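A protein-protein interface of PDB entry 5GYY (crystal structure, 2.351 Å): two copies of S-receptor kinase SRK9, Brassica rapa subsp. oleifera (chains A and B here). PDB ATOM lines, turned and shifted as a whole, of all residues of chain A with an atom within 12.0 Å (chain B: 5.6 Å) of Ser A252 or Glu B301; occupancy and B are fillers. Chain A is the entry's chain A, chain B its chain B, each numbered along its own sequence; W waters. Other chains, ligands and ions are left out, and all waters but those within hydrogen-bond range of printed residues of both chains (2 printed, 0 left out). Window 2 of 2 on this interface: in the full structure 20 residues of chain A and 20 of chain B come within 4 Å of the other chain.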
ATOM      1  N   LEU A  50      22.282  -9.686   2.325  1.00  0.00           N
ATOM      2  CA  LEU A  50      21.649  -8.506   2.903  1.00  0.00           C
ATOM      3  C   LEU A  50      20.130  -8.705   2.909  1.00  0.00           C
ATOM      4  O   LEU A  50      19.543  -9.012   1.872  1.00  0.00           O
ATOM      5  CB  LEU A  50      21.999  -7.256   2.096  1.00  0.00           C
ATOM      6  CG  LEU A  50      23.464  -6.872   1.949  1.00  0.00           C
ATOM      7  CD1 LEU A  50      23.566  -5.531   1.234  1.00  0.00           C
ATOM      8  CD2 LEU A  50      24.155  -6.831   3.309  1.00  0.00           C
ATOM      9  N   SER A  51      19.503  -8.577   4.074  1.00  0.00           N
ATOM     10  CA  SER A  51      18.049  -8.745   4.193  1.00  0.00           C
ATOM     11  C   SER A  51      17.226  -7.638   3.524  1.00  0.00           C
ATOM     12  O   SER A  51      16.129  -7.887   3.021  1.00  0.00           O
ATOM     13  CB  SER A  51      17.639  -8.885   5.663  1.00  0.00           C
ATOM     14  OG  SER A  51      17.986  -7.729   6.396  1.00  0.00           O
ATOM     15  N   SER A 208      40.805   1.518   2.780  1.00  0.00           N
ATOM     16  CA  SER A 208      41.426   0.313   3.296  1.00  0.00           C
ATOM     17  C   SER A 208      40.828  -0.940   2.653  1.00  0.00           C
ATOM     18  O   SER A 208      41.442  -1.998   2.673  1.00  0.00           O
ATOM     19  CB  SER A 208      41.322   0.259   4.828  1.00  0.00           C
ATOM     20  OG  SER A 208      39.973   0.258   5.281  1.00  0.00           O
ATOM     21  N   TYR A 209      39.627  -0.817   2.091  1.00  0.00           N
ATOM     22  CA  TYR A 209      38.931  -1.975   1.529  1.00  0.00           C
ATOM     23  C   TYR A 209      38.656  -1.890   0.024  1.00  0.00           C
ATOM     24  O   TYR A 209      38.093  -2.828  -0.561  1.00  0.00           O
ATOM     25  CB  TYR A 209      37.622  -2.222   2.288  1.00  0.00           C
ATOM     26  CG  TYR A 209      36.648  -1.067   2.210  1.00  0.00           C
ATOM     27  CD1 TYR A 209      35.720  -0.983   1.169  1.00  0.00           C
ATOM     28  CD2 TYR A 209      36.687  -0.038   3.140  1.00  0.00           C
ATOM     29  CE1 TYR A 209      34.835   0.067   1.085  1.00  0.00           C
ATOM     30  CE2 TYR A 209      35.804   1.026   3.063  1.00  0.00           C
ATOM     31  CZ  TYR A 209      34.876   1.073   2.036  1.00  0.00           C
ATOM     32  OH  TYR A 209      33.991   2.124   1.949  1.00  0.00           O
ATOM     33  N   SER A 231      34.353  -9.384   2.818  1.00  0.00           N
ATOM     34  CA  SER A 231      33.217  -9.254   3.721  1.00  0.00           C
ATOM     35  C   SER A 231      32.559  -7.884   3.597  1.00  0.00           C
ATOM     36  O   SER A 231      31.548  -7.609   4.247  1.00  0.00           O
ATOM     37  CB  SER A 231      33.660  -9.504   5.155  1.00  0.00           C
ATOM     38  OG  SER A 231      34.774  -8.689   5.456  1.00  0.00           O
ATOM     39  N   ILE A 232      33.142  -7.036   2.752  1.00  0.00           N
ATOM     40  CA  ILE A 232      32.651  -5.679   2.546  1.00  0.00           C
ATOM     41  C   ILE A 232      32.001  -5.429   1.168  1.00  0.00           C
ATOM     42  O   ILE A 232      32.551  -5.808   0.125  1.00  0.00           O
ATOM     43  CB  ILE A 232      33.776  -4.670   2.792  1.00  0.00           C
ATOM     44  CG1 ILE A 232      34.291  -4.833   4.224  1.00  0.00           C
ATOM     45  CG2 ILE A 232      33.301  -3.250   2.490  1.00  0.00           C
ATOM     46  CD1 ILE A 232      35.344  -3.838   4.616  1.00  0.00           C
ATOM     47  N   TYR A 233      30.821  -4.806   1.176  1.00  0.00           N
ATOM     48  CA  TYR A 233      30.144  -4.440  -0.055  1.00  0.00           C
ATOM     49  C   TYR A 233      30.228  -2.938  -0.310  1.00  0.00           C
ATOM     50  O   TYR A 233      29.771  -2.139   0.504  1.00  0.00           O
ATOM     51  CB  TYR A 233      28.674  -4.885  -0.037  1.00  0.00           C
ATOM     52  CG  TYR A 233      28.449  -6.342   0.333  1.00  0.00           C
ATOM     53  CD1 TYR A 233      29.373  -7.332   0.011  1.00  0.00           C
ATOM     54  CD2 TYR A 233      27.320  -6.718   1.031  1.00  0.00           C
ATOM     55  CE1 TYR A 233      29.151  -8.659   0.370  1.00  0.00           C
ATOM     56  CE2 TYR A 233      27.096  -8.026   1.387  1.00  0.00           C
ATOM     57  CZ  TYR A 233      28.003  -8.990   1.066  1.00  0.00           C
ATOM     58  OH  TYR A 233      27.740 -10.286   1.444  1.00  0.00           O
ATOM     59  N   THR A 248      28.751   2.184   0.650  1.00  0.00           N
ATOM     60  CA  THR A 248      29.366   1.050   1.313  1.00  0.00           C
ATOM     61  C   THR A 248      28.407   0.613   2.420  1.00  0.00           C
ATOM     62  O   THR A 248      27.984   1.426   3.256  1.00  0.00           O
ATOM     63  CB  THR A 248      30.767   1.441   1.877  1.00  0.00           C
ATOM     64  OG1 THR A 248      31.639   1.769   0.789  1.00  0.00           O
ATOM     65  CG2 THR A 248      31.383   0.308   2.687  1.00  0.00           C
ATOM     66  N   TRP A 249      28.045  -0.664   2.404  1.00  0.00           N
ATOM     67  CA  TRP A 249      27.152  -1.202   3.413  1.00  0.00           C
ATOM     68  C   TRP A 249      27.854  -1.223   4.761  1.00  0.00           C
ATOM     69  O   TRP A 249      28.880  -1.885   4.917  1.00  0.00           O
ATOM     70  CB  TRP A 249      26.668  -2.611   3.048  1.00  0.00           C
ATOM     71  CG  TRP A 249      25.799  -3.229   4.132  1.00  0.00           C
ATOM     72  CD1 TRP A 249      26.146  -4.225   5.004  1.00  0.00           C
ATOM     73  CD2 TRP A 249      24.450  -2.866   4.455  1.00  0.00           C
ATOM     74  NE1 TRP A 249      25.089  -4.515   5.834  1.00  0.00           N
ATOM     75  CE2 TRP A 249      24.037  -3.693   5.520  1.00  0.00           C
ATOM     76  CE3 TRP A 249      23.551  -1.922   3.944  1.00  0.00           C
ATOM     77  CZ2 TRP A 249      22.763  -3.596   6.093  1.00  0.00           C
ATOM     78  CZ3 TRP A 249      22.279  -1.832   4.506  1.00  0.00           C
ATOM     79  CH2 TRP A 249      21.902  -2.662   5.574  1.00  0.00           C
ATOM     80  N   THR A 250      27.288  -0.509   5.730  1.00  0.00           N
ATOM     81  CA  THR A 250      27.884  -0.399   7.056  1.00  0.00           C
ATOM     82  C   THR A 250      26.928  -0.990   8.095  1.00  0.00           C
ATOM     83  O   THR A 250      25.946  -0.360   8.458  1.00  0.00           O
ATOM     84  CB  THR A 250      28.109   1.063   7.392  1.00  0.00           C
ATOM     85  OG1 THR A 250      28.595   1.731   6.230  1.00  0.00           O
ATOM     86  CG2 THR A 250      29.091   1.233   8.561  1.00  0.00           C
ATOM     87  N   PRO A 251      27.220  -2.205   8.572  1.00  0.00           N
ATOM     88  CA  PRO A 251      26.348  -2.927   9.500  1.00  0.00           C
ATOM     89  C   PRO A 251      25.921  -2.094  10.707  1.00  0.00           C
ATOM     90  O   PRO A 251      24.727  -2.091  11.053  1.00  0.00           O
ATOM     91  CB  PRO A 251      27.220  -4.110   9.936  1.00  0.00           C
ATOM     92  CG  PRO A 251      28.065  -4.378   8.759  1.00  0.00           C
ATOM     93  CD  PRO A 251      28.360  -3.028   8.137  1.00  0.00           C
ATOM     94  N   SER A 252      26.868  -1.375  11.309  1.00  0.00           N
ATOM     95  CA  SER A 252      26.597  -0.611  12.519  1.00  0.00           C
ATOM     96  C   SER A 252      25.621   0.532  12.256  1.00  0.00           C
ATOM     97  O   SER A 252      24.973   1.021  13.181  1.00  0.00           O
ATOM     98  CB  SER A 252      27.896  -0.080  13.154  1.00  0.00           C
ATOM     99  OG  SER A 252      28.443   0.991  12.406  1.00  0.00           O
ATOM    100  N   LEU A 253      25.532   0.959  10.999  1.00  0.00           N
ATOM    101  CA  LEU A 253      24.561   1.977  10.599  1.00  0.00           C
ATOM    102  C   LEU A 253      23.277   1.368  10.049  1.00  0.00           C
ATOM    103  O   LEU A 253      22.279   2.072   9.911  1.00  0.00           O
ATOM    104  CB  LEU A 253      25.143   2.941   9.565  1.00  0.00           C
ATOM    105  CG  LEU A 253      26.174   3.958  10.041  1.00  0.00           C
ATOM    106  CD1 LEU A 253      26.745   4.720   8.863  1.00  0.00           C
ATOM    107  CD2 LEU A 253      25.544   4.930  11.034  1.00  0.00           C
ATOM    108  N   VAL A 254      23.303   0.071   9.737  1.00  0.00           N
ATOM    109  CA  VAL A 254      22.174  -0.598   9.073  1.00  0.00           C
ATOM    110  C   VAL A 254      21.753   0.186   7.837  1.00  0.00           C
ATOM    111  O   VAL A 254      20.585   0.538   7.681  1.00  0.00           O
ATOM    112  CB  VAL A 254      20.927  -0.750   9.990  1.00  0.00           C
ATOM    113  CG1 VAL A 254      20.040  -1.883   9.485  1.00  0.00           C
ATOM    114  CG2 VAL A 254      21.335  -0.985  11.446  1.00  0.00           C
ATOM    115  N   ILE A 255      22.712   0.540   6.996  1.00  0.00           N
ATOM    116  CA  ILE A 255      22.377   1.374   5.859  1.00  0.00           C
ATOM    117  C   ILE A 255      23.493   1.304   4.838  1.00  0.00           C
ATOM    118  O   ILE A 255      24.640   0.979   5.162  1.00  0.00           O
ATOM    119  CB  ILE A 255      22.092   2.855   6.286  1.00  0.00           C
ATOM    120  CG1 ILE A 255      21.007   3.495   5.408  1.00  0.00           C
ATOM    121  CG2 ILE A 255      23.378   3.676   6.359  1.00  0.00           C
ATOM    122  CD1 ILE A 255      20.636   4.917   5.804  1.00  0.00           C
ATOM    123  N   TRP A 256      23.134   1.567   3.595  1.00  0.00           N
ATOM    124  CA  TRP A 256      24.117   1.810   2.574  1.00  0.00           C
ATOM    125  C   TRP A 256      24.664   3.214   2.790  1.00  0.00           C
ATOM    126  O   TRP A 256      24.016   4.201   2.457  1.00  0.00           O
ATOM    127  CB  TRP A 256      23.490   1.631   1.189  1.00  0.00           C
ATOM    128  CG  TRP A 256      23.401   0.198   0.760  1.00  0.00           C
ATOM    129  CD1 TRP A 256      22.318  -0.636   0.857  1.00  0.00           C
ATOM    130  CD2 TRP A 256      24.452  -0.573   0.149  1.00  0.00           C
ATOM    131  NE1 TRP A 256      22.630  -1.880   0.338  1.00  0.00           N
ATOM    132  CE2 TRP A 256      23.932  -1.870  -0.097  1.00  0.00           C
ATOM    133  CE3 TRP A 256      25.781  -0.294  -0.207  1.00  0.00           C
ATOM    134  CZ2 TRP A 256      24.695  -2.885  -0.690  1.00  0.00           C
ATOM    135  CZ3 TRP A 256      26.548  -1.308  -0.789  1.00  0.00           C
ATOM    136  CH2 TRP A 256      25.995  -2.585  -1.031  1.00  0.00           C
ATOM    137  N   ASN A 257      25.870   3.291   3.351  1.00  0.00           N
ATOM    138  CA  ASN A 257      26.447   4.561   3.735  1.00  0.00           C
ATOM    139  C   ASN A 257      27.055   5.288   2.543  1.00  0.00           C
ATOM    140  O   ASN A 257      27.901   4.737   1.832  1.00  0.00           O
ATOM    141  CB  ASN A 257      27.500   4.357   4.825  1.00  0.00           C
ATOM    142  CG  ASN A 257      27.935   5.659   5.462  1.00  0.00           C
ATOM    143  OD1 ASN A 257      27.188   6.637   5.473  1.00  0.00           O
ATOM    144  ND2 ASN A 257      29.152   5.681   5.994  1.00  0.00           N
ATOM    145  N   PRO A 258      26.607   6.528   2.301  1.00  0.00           N
ATOM    146  CA  PRO A 258      27.169   7.315   1.189  1.00  0.00           C
ATOM    147  C   PRO A 258      28.556   7.886   1.512  1.00  0.00           C
ATOM    148  O   PRO A 258      28.696   8.872   2.227  1.00  0.00           O
ATOM    149  CB  PRO A 258      26.143   8.437   0.998  1.00  0.00           C
ATOM    150  CG  PRO A 258      25.419   8.513   2.318  1.00  0.00           C
ATOM    151  CD  PRO A 258      25.426   7.159   2.913  1.00  0.00           C
ATOM    152  N   ILE A 259      29.580   7.237   0.973  1.00  0.00           N
ATOM    153  CA  ILE A 259      30.956   7.700   1.086  1.00  0.00           C
ATOM    154  C   ILE A 259      31.102   9.048   0.390  1.00  0.00           C
ATOM    155  O   ILE A 259      31.788   9.939   0.888  1.00  0.00           O
ATOM    156  CB  ILE A 259      31.903   6.664   0.476  1.00  0.00           C
ATOM    157  CG1 ILE A 259      31.664   5.305   1.137  1.00  0.00           C
ATOM    158  CG2 ILE A 259      33.354   7.093   0.591  1.00  0.00           C
ATOM    159  CD1 ILE A 259      31.709   5.334   2.645  1.00  0.00           C
ATOM    160  N   ASN B 298      33.570   5.136  19.834  1.00  0.00           N
ATOM    161  CA  ASN B 298      33.706   3.835  19.181  1.00  0.00           C
ATOM    162  C   ASN B 298      34.528   3.982  17.891  1.00  0.00           C
ATOM    163  O   ASN B 298      34.005   4.413  16.853  1.00  0.00           O
ATOM    164  CB  ASN B 298      32.326   3.218  18.911  1.00  0.00           C
ATOM    165  CG  ASN B 298      32.407   1.760  18.479  1.00  0.00           C
ATOM    166  OD1 ASN B 298      33.369   1.342  17.849  1.00  0.00           O
ATOM    167  ND2 ASN B 298      31.395   0.983  18.829  1.00  0.00           N
ATOM    168  N   VAL B 299      35.816   3.633  17.980  1.00  0.00           N
ATOM    169  CA  VAL B 299      36.783   3.873  16.907  1.00  0.00           C
ATOM    170  C   VAL B 299      36.494   3.048  15.648  1.00  0.00           C
ATOM    171  O   VAL B 299      36.626   3.542  14.529  1.00  0.00           O
ATOM    172  CB  VAL B 299      38.226   3.588  17.383  1.00  0.00           C
ATOM    173  CG1 VAL B 299      39.218   4.320  16.498  1.00  0.00           C
ATOM    174  CG2 VAL B 299      38.398   4.049  18.809  1.00  0.00           C
ATOM    175  N   GLN B 300      36.097   1.795  15.846  1.00  0.00           N
ATOM    176  CA  GLN B 300      35.765   0.893  14.749  1.00  0.00           C
ATOM    177  C   GLN B 300      34.579   1.457  13.968  1.00  0.00           C
ATOM    178  O   GLN B 300      34.564   1.421  12.741  1.00  0.00           O
ATOM    179  CB  GLN B 300      35.432  -0.510  15.274  1.00  0.00           C
ATOM    180  CG  GLN B 300      36.616  -1.279  15.873  1.00  0.00           C
ATOM    181  CD  GLN B 300      37.096  -0.709  17.214  1.00  0.00           C
ATOM    182  OE1 GLN B 300      36.290  -0.360  18.091  1.00  0.00           O
ATOM    183  NE2 GLN B 300      38.417  -0.619  17.378  1.00  0.00           N
ATOM    184  N   GLU B 301      33.584   1.981  14.680  1.00  0.00           N
ATOM    185  CA  GLU B 301      32.499   2.707  14.033  1.00  0.00           C
ATOM    186  C   GLU B 301      33.008   3.992  13.382  1.00  0.00           C
ATOM    187  O   GLU B 301      32.620   4.324  12.263  1.00  0.00           O
ATOM    188  CB  GLU B 301      31.378   3.028  15.030  1.00  0.00           C
ATOM    189  CG  GLU B 301      30.541   1.822  15.409  1.00  0.00           C
ATOM    190  CD  GLU B 301      29.488   2.134  16.446  1.00  0.00           C
ATOM    191  OE1 GLU B 301      29.519   3.248  17.013  1.00  0.00           O
ATOM    192  OE2 GLU B 301      28.628   1.262  16.696  1.00  0.00           O
ATOM    193  N   TRP B 302      33.886   4.704  14.083  1.00  0.00           N
ATOM    194  CA  TRP B 302      34.432   5.967  13.588  1.00  0.00           C
ATOM    195  C   TRP B 302      35.204   5.793  12.284  1.00  0.00           C
ATOM    196  O   TRP B 302      35.137   6.644  11.399  1.00  0.00           O
ATOM    197  CB  TRP B 302      35.334   6.622  14.640  1.00  0.00           C
ATOM    198  CG  TRP B 302      35.507   8.095  14.433  1.00  0.00           C
ATOM    199  CD1 TRP B 302      36.533   8.730  13.771  1.00  0.00           C
ATOM    200  CD2 TRP B 302      34.607   9.122  14.859  1.00  0.00           C
ATOM    201  NE1 TRP B 302      36.317  10.090  13.772  1.00  0.00           N
ATOM    202  CE2 TRP B 302      35.143  10.353  14.432  1.00  0.00           C
ATOM    203  CE3 TRP B 302      33.391   9.116  15.554  1.00  0.00           C
ATOM    204  CZ2 TRP B 302      34.510  11.569  14.689  1.00  0.00           C
ATOM    205  CZ3 TRP B 302      32.762  10.320  15.804  1.00  0.00           C
ATOM    206  CH2 TRP B 302      33.324  11.531  15.378  1.00  0.00           C
ATOM    207  N   ASP B 303      35.949   4.700  12.170  1.00  0.00           N
ATOM    208  CA  ASP B 303      36.717   4.443  10.954  1.00  0.00           C
ATOM    209  C   ASP B 303      35.805   4.060   9.788  1.00  0.00           C
ATOM    210  O   ASP B 303      36.121   4.318   8.628  1.00  0.00           O
ATOM    211  CB  ASP B 303      37.769   3.358  11.193  1.00  0.00           C
ATOM    212  CG  ASP B 303      38.825   3.781  12.202  1.00  0.00           C
ATOM    213  OD1 ASP B 303      38.991   5.003  12.421  1.00  0.00           O
ATOM    214  OD2 ASP B 303      39.475   2.885  12.784  1.00  0.00           O
ATOM    215  N   MET B 304      34.655   3.472  10.107  1.00  0.00           N
ATOM    216  CA  MET B 304      33.668   3.125   9.096  1.00  0.00           C
ATOM    217  C   MET B 304      32.745   4.304   8.794  1.00  0.00           C
ATOM    218  O   MET B 304      31.714   4.148   8.137  1.00  0.00           O
ATOM    219  CB  MET B 304      32.851   1.921   9.557  1.00  0.00           C
ATOM    220  CG  MET B 304      33.539   0.586   9.345  1.00  0.00           C
ATOM    221  SD  MET B 304      33.909   0.342   7.593  1.00  0.00           S
ATOM    222  CE  MET B 304      35.178  -0.932   7.687  1.00  0.00           C
ATOM    223  N   ARG B 305      33.146   5.485   9.266  1.00  0.00           N
ATOM    224  CA  ARG B 305      32.375   6.725   9.127  1.00  0.00           C
ATOM    225  C   ARG B 305      30.952   6.612   9.726  1.00  0.00           C
ATOM    226  O   ARG B 305      29.991   7.189   9.209  1.00  0.00           O
ATOM    227  CB  ARG B 305      32.379   7.257   7.680  1.00  0.00           C
ATOM    228  CG  ARG B 305      33.749   7.779   7.213  1.00  0.00           C
ATOM    229  CD  ARG B 305      33.762   8.113   5.736  1.00  0.00           C
ATOM    230  NE  ARG B 305      32.838   9.200   5.412  1.00  0.00           N
ATOM    231  CZ  ARG B 305      32.647   9.690   4.186  1.00  0.00           C
ATOM    232  NH1 ARG B 305      33.295   9.172   3.143  1.00  0.00           N
ATOM    233  NH2 ARG B 305      31.779  10.681   3.993  1.00  0.00           N
ATOM    234  N   ASP B 306      30.847   5.842  10.810  1.00  0.00           N
ATOM    235  CA  ASP B 306      29.668   5.819  11.669  1.00  0.00           C
ATOM    236  C   ASP B 306      29.966   6.742  12.864  1.00  0.00           C
ATOM    237  O   ASP B 306      30.669   6.373  13.816  1.00  0.00           O
ATOM    238  CB  ASP B 306      29.403   4.384  12.120  1.00  0.00           C
ATOM    239  CG  ASP B 306      28.204   4.258  13.043  1.00  0.00           C
ATOM    240  OD1 ASP B 306      27.751   5.280  13.604  1.00  0.00           O
ATOM    241  OD2 ASP B 306      27.697   3.120  13.179  1.00  0.00           O
ATOM    242  N   HIS B 307      29.433   7.953  12.804  1.00  0.00           N
ATOM    243  CA  HIS B 307      29.807   8.958  13.774  1.00  0.00           C
ATOM    244  C   HIS B 307      28.764   9.176  14.880  1.00  0.00           C
ATOM    245  O   HIS B 307      28.855  10.136  15.644  1.00  0.00           O
ATOM    246  CB  HIS B 307      30.117  10.267  13.050  1.00  0.00           C
ATOM    247  CG  HIS B 307      31.193  10.134  12.016  1.00  0.00           C
ATOM    248  ND1 HIS B 307      32.497   9.833  12.343  1.00  0.00           N
ATOM    249  CD2 HIS B 307      31.162  10.279  10.668  1.00  0.00           C
ATOM    250  CE1 HIS B 307      33.224   9.793  11.243  1.00  0.00           C
ATOM    251  NE2 HIS B 307      32.441  10.063  10.216  1.00  0.00           N
ATOM    252  N   ARG B 309      27.754   7.853  17.854  1.00  0.00           N
ATOM    253  CA  ARG B 309      28.018   7.927  19.283  1.00  0.00           C
ATOM    254  C   ARG B 309      28.792   9.169  19.661  1.00  0.00           C
ATOM    255  O   ARG B 309      28.804   9.555  20.820  1.00  0.00           O
ATOM    256  CB  ARG B 309      28.742   6.670  19.775  1.00  0.00           C
ATOM    257  CG  ARG B 309      28.004   5.391  19.446  1.00  0.00           C
ATOM    258  CD  ARG B 309      28.725   4.151  19.945  1.00  0.00           C
ATOM    259  NE  ARG B 309      27.950   2.968  19.576  1.00  0.00           N
ATOM    260  CZ  ARG B 309      27.937   1.836  20.263  1.00  0.00           C
ATOM    261  NH1 ARG B 309      28.674   1.723  21.357  1.00  0.00           N
ATOM    262  NH2 ARG B 309      27.194   0.818  19.859  1.00  0.00           N
HETATM  263  O   HOH W   1      31.253  12.762   1.876  1.00  0.00           O
HETATM  264  O   HOH W   2      30.815   3.245   5.835  1.00  0.00           O
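The guanidinium group (NH1) of Arg B305 is in hydrogen-bond range of the backbone carbonyl oxygen (O) of Ile A259 (2.8 Å). OG of Ser A252 sits close to OD2 of Asp B306 (2.4 Å).
The side-chain hydroxyl of Thr A250 is in hydrogen-bond range of the backbone carbonyl oxygen of Thr A248, at 3.1 Å. The backbone carbonyl oxygen of Thr A248 is in hydrogen-bond range of the backbone NH of Asn A257. The backbone NH (N) of Thr A250 is in hydrogen-bond range of the backbone carbonyl oxygen (O) of Ile A255 (3.1 Å). The side-chain amide oxygen (OD1) of Asn B298 lies within hydrogen-bond range of the backbone NH (N) of Glu B301 (3.2 Å). O of Glu B301 lies within hydrogen-bond range of N of Asp B306 (2.7 Å). The side-chain carboxylate (OE1) of Glu B301 is in salt-bridge range of the guanidinium group (NE) of Arg B309 (3.0 Å).
Thr A250 touches Met B304. Glu B301 touches Ser A252 (CG to OG, 3.8 Å). Leu A253 touches Asp B306 (CD2 to CG, 3.4 Å). Asn A257 touches Met B304. ND2 of Asn A257 touches O of Arg B305, at 3.6 Å. Pro A258 touches Arg B305.
Of chain B, only Glu B301 and Asp B306 come within 4 Å of Ser A252. Printed residues of chain B within 4 Å of Leu A253: Asp B306. Of the printed residues of chain B, Pro A258 touches Arg B305 (3.99 Å). Of the printed residues of chain B, Ile A259 touches Arg B305. No residue of chain A comes within 4 Å of Val B299. Gln B300 touches none of the printed residues of chain A. Glu B301 touches just one residue of chain A: Ser A252 (3.8 Å). No residue of chain A comes within 4 Å of Trp B302. No residue of chain A comes within 4 Å of Asp B303. Met B304 touches just these residues of chain A: Thr A250 (3.9 Å) and Asn A257 (3.7 Å). Asp B306 touches just these residues of chain A: Ser A252 (2.4 Å) and Leu A253 (3.4 Å). No residue of chain A comes within 4 Å of Arg B309.
Of the 11 printed residues of chain B, 4 touch a printed residue of chain A. Printed residues of chain B that touch a printed residue of chain A: Glu B301, Met B304, Arg B305 and Asp B306. Hydrophobic or aromatic side chains of chain B within 4 Å of the printed part of chain A: Met B304. Among the printed residues, no Asp or Glu carboxylate lies within 4 Å of a Lys or Arg side-chain nitrogen of the other chain.
No position is printed for both chains. Of the 8 pairs that touch across the chains among the printed residues, none has its exchanged pair printed and touching as well.
Water W2 lies within hydrogen-bond range of the backbone carbonyl oxygen of Met B304, the side-chain hydroxyl of Thr A250 and the side-chain amide nitrogen of Asn A257. Water W1 lies within hydrogen-bond range of NH2 of Arg B305 and O of Ile A259.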
